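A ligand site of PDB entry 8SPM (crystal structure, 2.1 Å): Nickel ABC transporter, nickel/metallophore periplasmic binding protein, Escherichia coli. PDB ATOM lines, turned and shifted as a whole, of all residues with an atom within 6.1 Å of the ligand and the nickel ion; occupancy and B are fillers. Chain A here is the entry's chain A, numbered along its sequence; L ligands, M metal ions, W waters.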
ATOM      1  N   TYR A  21      -8.246  -8.822  18.939  1.00  0.00           N
ATOM      2  CA  TYR A  21      -7.801  -9.254  17.611  1.00  0.00           C
ATOM      3  C   TYR A  21      -7.376  -8.020  16.793  1.00  0.00           C
ATOM      4  O   TYR A  21      -6.877  -7.039  17.372  1.00  0.00           O
ATOM      5  CB  TYR A  21      -8.915 -10.082  16.976  1.00  0.00           C
ATOM      6  CG  TYR A  21      -9.175 -11.318  17.833  1.00  0.00           C
ATOM      7  CD1 TYR A  21     -10.059 -11.265  18.961  1.00  0.00           C
ATOM      8  CD2 TYR A  21      -8.487 -12.497  17.592  1.00  0.00           C
ATOM      9  CE1 TYR A  21     -10.244 -12.383  19.766  1.00  0.00           C
ATOM     10  CE2 TYR A  21      -8.677 -13.622  18.376  1.00  0.00           C
ATOM     11  CZ  TYR A  21      -9.564 -13.576  19.454  1.00  0.00           C
ATOM     12  OH  TYR A  21      -9.723 -14.737  20.208  1.00  0.00           O
ATOM     13  N   THR A  22      -7.518  -8.089  15.479  1.00  0.00           N
ATOM     14  CA  THR A  22      -7.201  -6.935  14.657  1.00  0.00           C
ATOM     15  C   THR A  22      -7.950  -5.742  15.234  1.00  0.00           C
ATOM     16  O   THR A  22      -9.137  -5.877  15.588  1.00  0.00           O
ATOM     17  CB  THR A  22      -7.559  -7.190  13.173  1.00  0.00           C
ATOM     18  OG1 THR A  22      -6.790  -6.341  12.320  1.00  0.00           O
ATOM     19  CG2 THR A  22      -9.040  -6.940  12.843  1.00  0.00           C
ATOM     20  N   PRO A  23      -7.297  -4.595  15.400  1.00  0.00           N
ATOM     21  CA  PRO A  23      -5.991  -4.195  14.848  1.00  0.00           C
ATOM     22  C   PRO A  23      -4.694  -4.673  15.560  1.00  0.00           C
ATOM     23  O   PRO A  23      -3.615  -4.367  15.026  1.00  0.00           O
ATOM     24  CB  PRO A  23      -6.057  -2.655  14.909  1.00  0.00           C
ATOM     25  CG  PRO A  23      -7.065  -2.355  16.030  1.00  0.00           C
ATOM     26  CD  PRO A  23      -8.089  -3.434  15.892  1.00  0.00           C
ATOM     27  N   ASN A  24      -4.776  -5.361  16.700  1.00  0.00           N
ATOM     28  CA  ASN A  24      -3.571  -5.939  17.308  1.00  0.00           C
ATOM     29  C   ASN A  24      -2.891  -6.940  16.374  1.00  0.00           C
ATOM     30  O   ASN A  24      -3.546  -7.850  15.857  1.00  0.00           O
ATOM     31  CB  ASN A  24      -3.924  -6.652  18.608  1.00  0.00           C
ATOM     32  CG  ASN A  24      -4.594  -5.744  19.603  1.00  0.00           C
ATOM     33  OD1 ASN A  24      -3.935  -4.921  20.233  1.00  0.00           O
ATOM     34  ND2 ASN A  24      -5.903  -5.870  19.753  1.00  0.00           N
ATOM     35  N   MET A  26      -0.403 -10.054  15.652  1.00  0.00           N
ATOM     36  CA  MET A  26      -0.073 -11.220  16.467  1.00  0.00           C
ATOM     37  C   MET A  26       1.423 -11.293  16.776  1.00  0.00           C
ATOM     38  O   MET A  26       1.808 -11.644  17.904  1.00  0.00           O
ATOM     39  CB  MET A  26      -0.562 -12.497  15.777  1.00  0.00           C
ATOM     40  CG  MET A  26      -2.088 -12.669  15.893  1.00  0.00           C
ATOM     41  SD  MET A  26      -2.795 -13.894  14.770  1.00  0.00           S
ATOM     42  CE  MET A  26      -2.662 -15.294  15.876  1.00  0.00           C
ATOM     43  N   ARG A  96     -16.627 -13.693  22.154  1.00  0.00           N
ATOM     44  CA  ARG A  96     -15.679 -13.227  21.139  1.00  0.00           C
ATOM     45  C   ARG A  96     -14.669 -14.308  20.763  1.00  0.00           C
ATOM     46  O   ARG A  96     -14.053 -14.221  19.689  1.00  0.00           O
ATOM     47  CB  ARG A  96     -14.948 -11.982  21.645  1.00  0.00           C
ATOM     48  CG  ARG A  96     -14.040 -11.350  20.606  1.00  0.00           C
ATOM     49  CD  ARG A  96     -14.827 -10.928  19.382  1.00  0.00           C
ATOM     50  NE  ARG A  96     -13.937 -10.352  18.362  1.00  0.00           N
ATOM     51  CZ  ARG A  96     -13.238 -11.057  17.489  1.00  0.00           C
ATOM     52  NH1 ARG A  96     -13.263 -12.387  17.478  1.00  0.00           N
ATOM     53  NH2 ARG A  96     -12.467 -10.421  16.601  1.00  0.00           N
ATOM     54  N   TRP A  99     -14.745 -19.014  18.403  1.00  0.00           N
ATOM     55  CA  TRP A  99     -14.093 -19.714  17.294  1.00  0.00           C
ATOM     56  C   TRP A  99     -13.094 -20.755  17.788  1.00  0.00           C
ATOM     57  O   TRP A  99     -12.892 -21.777  17.131  1.00  0.00           O
ATOM     58  CB  TRP A  99     -13.390 -18.719  16.358  1.00  0.00           C
ATOM     59  CG  TRP A  99     -12.279 -18.012  17.086  1.00  0.00           C
ATOM     60  CD1 TRP A  99     -12.373 -16.905  17.871  1.00  0.00           C
ATOM     61  CD2 TRP A  99     -10.913 -18.437  17.148  1.00  0.00           C
ATOM     62  NE1 TRP A  99     -11.132 -16.578  18.405  1.00  0.00           N
ATOM     63  CE2 TRP A  99     -10.221 -17.518  17.976  1.00  0.00           C
ATOM     64  CE3 TRP A  99     -10.189 -19.486  16.567  1.00  0.00           C
ATOM     65  CZ2 TRP A  99      -8.844 -17.613  18.226  1.00  0.00           C
ATOM     66  CZ3 TRP A  99      -8.822 -19.580  16.819  1.00  0.00           C
ATOM     67  CH2 TRP A  99      -8.162 -18.646  17.640  1.00  0.00           C
ATOM     68  N   ARG A 136      -2.776 -15.674  21.007  1.00  0.00           N
ATOM     69  CA  ARG A 136      -3.892 -15.052  21.711  1.00  0.00           C
ATOM     70  C   ARG A 136      -5.070 -16.018  21.679  1.00  0.00           C
ATOM     71  O   ARG A 136      -5.148 -16.853  20.775  1.00  0.00           O
ATOM     72  CB  ARG A 136      -4.286 -13.721  21.068  1.00  0.00           C
ATOM     73  CG  ARG A 136      -4.766 -13.878  19.609  1.00  0.00           C
ATOM     74  CD  ARG A 136      -4.792 -12.524  18.949  1.00  0.00           C
ATOM     75  NE  ARG A 136      -5.135 -12.568  17.525  1.00  0.00           N
ATOM     76  CZ  ARG A 136      -5.091 -11.506  16.745  1.00  0.00           C
ATOM     77  NH1 ARG A 136      -4.657 -10.344  17.191  1.00  0.00           N
ATOM     78  NH2 ARG A 136      -5.517 -11.597  15.493  1.00  0.00           N
ATOM     79  N   TYR A 381     -11.624  -8.147   6.741  1.00  0.00           N
ATOM     80  CA  TYR A 381     -12.015  -9.074   7.805  1.00  0.00           C
ATOM     81  C   TYR A 381     -13.484  -8.926   8.133  1.00  0.00           C
ATOM     82  O   TYR A 381     -14.202  -9.910   8.256  1.00  0.00           O
ATOM     83  CB  TYR A 381     -11.151  -8.878   9.054  1.00  0.00           C
ATOM     84  CG  TYR A 381      -9.764  -9.428   8.890  1.00  0.00           C
ATOM     85  CD1 TYR A 381      -9.568 -10.656   8.251  1.00  0.00           C
ATOM     86  CD2 TYR A 381      -8.650  -8.732   9.340  1.00  0.00           C
ATOM     87  CE1 TYR A 381      -8.309 -11.171   8.061  1.00  0.00           C
ATOM     88  CE2 TYR A 381      -7.385  -9.233   9.134  1.00  0.00           C
ATOM     89  CZ  TYR A 381      -7.229 -10.452   8.498  1.00  0.00           C
ATOM     90  OH  TYR A 381      -5.976 -10.973   8.287  1.00  0.00           O
ATOM     91  N   ARG A 385     -16.399 -11.720   7.936  1.00  0.00           N
ATOM     92  CA  ARG A 385     -17.214 -11.983   9.113  1.00  0.00           C
ATOM     93  C   ARG A 385     -18.706 -11.931   8.782  1.00  0.00           C
ATOM     94  O   ARG A 385     -19.484 -12.740   9.295  1.00  0.00           O
ATOM     95  CB  ARG A 385     -16.832 -10.974  10.173  1.00  0.00           C
ATOM     96  CG  ARG A 385     -17.188 -11.319  11.555  1.00  0.00           C
ATOM     97  CD  ARG A 385     -16.427 -10.406  12.541  1.00  0.00           C
ATOM     98  NE  ARG A 385     -16.480 -10.957  13.896  1.00  0.00           N
ATOM     99  CZ  ARG A 385     -15.636 -11.883  14.365  1.00  0.00           C
ATOM    100  NH1 ARG A 385     -14.683 -12.383  13.602  1.00  0.00           N
ATOM    101  NH2 ARG A 385     -15.768 -12.302  15.626  1.00  0.00           N
ATOM    102  N   THR A 396      -5.005 -20.511   5.262  1.00  0.00           N
ATOM    103  CA  THR A 396      -5.076 -21.252   6.537  1.00  0.00           C
ATOM    104  C   THR A 396      -4.062 -20.663   7.525  1.00  0.00           C
ATOM    105  O   THR A 396      -3.405 -19.632   7.272  1.00  0.00           O
ATOM    106  CB  THR A 396      -4.923 -22.765   6.324  1.00  0.00           C
ATOM    107  OG1 THR A 396      -3.623 -23.074   5.845  1.00  0.00           O
ATOM    108  CG2 THR A 396      -5.970 -23.281   5.316  1.00  0.00           C
ATOM    109  N   TRP A 397      -3.918 -21.300   8.691  1.00  0.00           N
ATOM    110  CA  TRP A 397      -3.327 -20.600   9.823  1.00  0.00           C
ATOM    111  C   TRP A 397      -1.983 -21.155  10.281  1.00  0.00           C
ATOM    112  O   TRP A 397      -1.412 -20.601  11.232  1.00  0.00           O
ATOM    113  CB  TRP A 397      -4.307 -20.606  10.995  1.00  0.00           C
ATOM    114  CG  TRP A 397      -5.499 -19.792  10.725  1.00  0.00           C
ATOM    115  CD1 TRP A 397      -5.650 -18.888   9.728  1.00  0.00           C
ATOM    116  CD2 TRP A 397      -6.726 -19.795  11.478  1.00  0.00           C
ATOM    117  NE1 TRP A 397      -6.902 -18.322   9.808  1.00  0.00           N
ATOM    118  CE2 TRP A 397      -7.585 -18.866  10.866  1.00  0.00           C
ATOM    119  CE3 TRP A 397      -7.171 -20.486  12.612  1.00  0.00           C
ATOM    120  CZ2 TRP A 397      -8.879 -18.629  11.342  1.00  0.00           C
ATOM    121  CZ3 TRP A 397      -8.466 -20.242  13.081  1.00  0.00           C
ATOM    122  CH2 TRP A 397      -9.292 -19.321  12.439  1.00  0.00           C
ATOM    123  N   TYR A 401      -2.704 -24.445  14.435  1.00  0.00           N
ATOM    124  CA  TYR A 401      -4.127 -24.327  14.161  1.00  0.00           C
ATOM    125  C   TYR A 401      -4.610 -25.381  13.161  1.00  0.00           C
ATOM    126  O   TYR A 401      -5.791 -25.803  13.223  1.00  0.00           O
ATOM    127  CB  TYR A 401      -4.456 -22.944  13.605  1.00  0.00           C
ATOM    128  CG  TYR A 401      -4.003 -21.766  14.418  1.00  0.00           C
ATOM    129  CD1 TYR A 401      -2.706 -21.257  14.308  1.00  0.00           C
ATOM    130  CD2 TYR A 401      -4.893 -21.093  15.235  1.00  0.00           C
ATOM    131  CE1 TYR A 401      -2.309 -20.146  15.032  1.00  0.00           C
ATOM    132  CE2 TYR A 401      -4.522 -19.980  15.936  1.00  0.00           C
ATOM    133  CZ  TYR A 401      -3.224 -19.500  15.840  1.00  0.00           C
ATOM    134  OH  TYR A 401      -2.875 -18.386  16.575  1.00  0.00           O
ATOM    135  N   SER A 409     -13.106 -22.919  13.937  1.00  0.00           N
ATOM    136  CA  SER A 409     -13.495 -21.549  13.556  1.00  0.00           C
ATOM    137  C   SER A 409     -14.607 -21.494  12.505  1.00  0.00           C
ATOM    138  O   SER A 409     -15.195 -20.428  12.296  1.00  0.00           O
ATOM    139  CB  SER A 409     -12.289 -20.818  12.993  1.00  0.00           C
ATOM    140  OG  SER A 409     -12.178 -21.090  11.576  1.00  0.00           O
ATOM    141  N   VAL A 412     -18.560 -20.521  13.681  1.00  0.00           N
ATOM    142  CA  VAL A 412     -19.072 -19.188  13.977  1.00  0.00           C
ATOM    143  C   VAL A 412     -18.462 -18.230  12.962  1.00  0.00           C
ATOM    144  O   VAL A 412     -17.514 -18.596  12.239  1.00  0.00           O
ATOM    145  CB  VAL A 412     -18.743 -18.755  15.436  1.00  0.00           C
ATOM    146  CG1 VAL A 412     -19.381 -19.704  16.422  1.00  0.00           C
ATOM    147  CG2 VAL A 412     -17.233 -18.700  15.656  1.00  0.00           C
ATOM    148  N   PRO A 413     -19.029 -17.046  12.816  1.00  0.00           N
ATOM    149  CA  PRO A 413     -18.337 -16.031  12.037  1.00  0.00           C
ATOM    150  C   PRO A 413     -16.935 -15.840  12.586  1.00  0.00           C
ATOM    151  O   PRO A 413     -16.741 -15.559  13.776  1.00  0.00           O
ATOM    152  CB  PRO A 413     -19.222 -14.777  12.219  1.00  0.00           C
ATOM    153  CG  PRO A 413     -20.603 -15.368  12.420  1.00  0.00           C
ATOM    154  CD  PRO A 413     -20.365 -16.607  13.249  1.00  0.00           C
ATOM    155  N   SER A 414     -15.925 -16.009  11.737  1.00  0.00           N
ATOM    156  CA  SER A 414     -14.559 -15.872  12.235  1.00  0.00           C
ATOM    157  C   SER A 414     -13.751 -15.234  11.120  1.00  0.00           C
ATOM    158  O   SER A 414     -13.742 -14.015  11.001  1.00  0.00           O
ATOM    159  CB  SER A 414     -14.013 -17.250  12.665  1.00  0.00           C
ATOM    160  OG  SER A 414     -12.611 -17.218  12.911  1.00  0.00           O
ATOM    161  N   HIS A 415     -13.097 -16.044  10.292  1.00  0.00           N
ATOM    162  CA  HIS A 415     -12.694 -15.561   8.988  1.00  0.00           C
ATOM    163  C   HIS A 415     -13.855 -15.866   8.020  1.00  0.00           C
ATOM    164  O   HIS A 415     -15.020 -15.797   8.425  1.00  0.00           O
ATOM    165  CB  HIS A 415     -11.320 -16.157   8.615  1.00  0.00           C
ATOM    166  CG  HIS A 415     -10.197 -15.608   9.466  1.00  0.00           C
ATOM    167  ND1 HIS A 415      -9.073 -15.015   8.935  1.00  0.00           N
ATOM    168  CD2 HIS A 415     -10.055 -15.518  10.818  1.00  0.00           C
ATOM    169  CE1 HIS A 415      -8.286 -14.592   9.910  1.00  0.00           C
ATOM    170  NE2 HIS A 415      -8.859 -14.881  11.071  1.00  0.00           N
ATOM    171  N   THR A 489       2.735 -16.969  12.668  1.00  0.00           N
ATOM    172  CA  THR A 489       2.610 -15.527  12.799  1.00  0.00           C
ATOM    173  C   THR A 489       3.619 -14.910  13.761  1.00  0.00           C
ATOM    174  O   THR A 489       3.633 -13.687  13.911  1.00  0.00           O
ATOM    175  CB  THR A 489       1.184 -15.141  13.253  1.00  0.00           C
ATOM    176  OG1 THR A 489       0.889 -15.806  14.489  1.00  0.00           O
ATOM    177  CG2 THR A 489       0.138 -15.500  12.176  1.00  0.00           C
HETATM  178  N1  LIG L   1      -9.644 -13.638  13.624  1.00  0.00           N
HETATM  179  C1  LIG L   1     -10.467 -14.763  14.061  1.00  0.00           C
HETATM  180  C2  LIG L   1      -9.544 -15.836  14.668  1.00  0.00           C
HETATM  181  O1  LIG L   1      -7.051 -13.958  14.502  1.00  0.00           O
HETATM  182  C3  LIG L   1      -7.172 -16.325  14.598  1.00  0.00           C
HETATM  183  C4  LIG L   1      -6.053 -16.931  13.734  1.00  0.00           C
HETATM  184  C5  LIG L   1      -5.553 -15.988  12.651  1.00  0.00           C
HETATM  185  N2  LIG L   1      -8.008 -12.467  12.253  1.00  0.00           N
HETATM  186  C6  LIG L   1      -9.282 -11.708  12.293  1.00  0.00           C
HETATM  187  O2  LIG L   1      -4.361 -16.340  12.160  1.00  0.00           O
HETATM  188  C7  LIG L   1     -10.322 -12.750  12.668  1.00  0.00           C
HETATM  189  C8  LIG L   1      -6.748 -14.972  15.132  1.00  0.00           C
HETATM  190  C9  LIG L   1     -11.720 -14.503  14.907  1.00  0.00           C
HETATM  191  C10 LIG L   1      -9.391 -10.589  13.344  1.00  0.00           C
HETATM  192  N3  LIG L   1      -8.375 -16.035  13.801  1.00  0.00           N
HETATM  193  O3  LIG L   1      -6.190 -15.016  12.262  1.00  0.00           O
HETATM  194  O4  LIG L   1      -6.017 -15.029  16.269  1.00  0.00           O
HETATM  195  O5  LIG L   1     -11.805 -13.294  15.415  1.00  0.00           O
HETATM  196  O6  LIG L   1     -12.590 -15.353  15.056  1.00  0.00           O
HETATM  197  O7  LIG L   1      -8.252 -10.129  13.862  1.00  0.00           O
HETATM  198  O8  LIG L   1     -10.496 -10.176  13.676  1.00  0.00           O
HETATM  199 NI    NI M   1      -7.995 -14.371  12.801  1.00  0.00          NI
HETATM  200  O   HOH W   1      -4.927 -17.232  17.689  1.00  0.00           O
HETATM  201  O   HOH W   2     -15.053 -15.026  15.960  1.00  0.00           O
HETATM  202  O   HOH W   3     -10.976  -8.000  15.026  1.00  0.00           O
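The guanidinium group (NH1) of Arg 385 is in hydrogen-bond range of the backbone carbonyl oxygen (O) of Ser 414, 3.2 Å away.
SD of Met 26 lies close to NH2 of Arg 136 (3.6 Å).
O of Asn 24 lies within hydrogen-bond range of NH1 of Arg 136 (3.0 Å).
The indole nitrogen of Trp 99 lies within hydrogen-bond range of the side-chain hydroxyl of Tyr 21 (2.9 Å).
The side-chain amide nitrogen (ND2) of Asn 24 sits at hydrogen-bond distance from the backbone carbonyl oxygen (O) of Tyr 21 (2.8 Å).
The backbone NH of Ser 409 sits at hydrogen-bond distance from the backbone carbonyl oxygen of Trp 99.
An oxygen (O5) of the ligand is in salt-bridge range of the guanidinium group (NH1) of Arg 96 (2.7 Å).
The backbone NH of Thr 22 lies within hydrogen-bond range of an oxygen (O7) of the ligand.
O6 of the ligand is in hydrogen-bond range of OG of Ser 414 (2.8 Å).
The guanidinium group (NE) of Arg 136 is in salt-bridge range of an oxygen (O4) of the ligand.
The guanidinium group of Arg 385 is in salt-bridge range of an oxygen (O5) of the ligand (3.5 Å).
An oxygen (O4) of the ligand sits close to the side-chain sulfur (SD) of Met 26 (3.7 Å).
Tyr 21 touches the ligand (CB to O7, 3.2 Å).
Trp 99 touches the ligand.
Trp 397 touches the ligand.
Hydrophobic or aromatic side chains that line the ligand: Tyr 21, Met 26, Trp 99, Trp 397 and His 415.
Water W3 lies within hydrogen-bond range of an oxygen (O8) of the ligand (2.6 Å), the backbone carbonyl oxygen of Thr 22 (2.9 Å) and the guanidinium group of Arg 96 (3.3 Å).
Water W2 lies within hydrogen-bond range of O6 of the ligand, O of Pro 413 and NH2 of Arg 385.
Water W1 lies within hydrogen-bond range of the side-chain hydroxyl of Tyr 401 (2.6 Å), an oxygen (O4) of the ligand (2.8 Å) and the backbone carbonyl oxygen of Arg 136 (3.1 Å).
The nickel ion is bound by a nitrogen (N3) of the ligand (2.0 Å).
The nickel ion is bound by a nitrogen (N2) of the ligand (2.0 Å).
A nitrogen (N1) of the ligand binds the nickel ion, 2.0 Å away.
The nickel ion is bound by O1 of the ligand (2.0 Å).
The nickel ion is bound by an oxygen (O3) of the ligand, 2.0 Å away.
NE2 of His 415 binds the nickel ion, at 2.0 Å.
One residue has an atom within 4 Å of the nickel ion: His 415.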
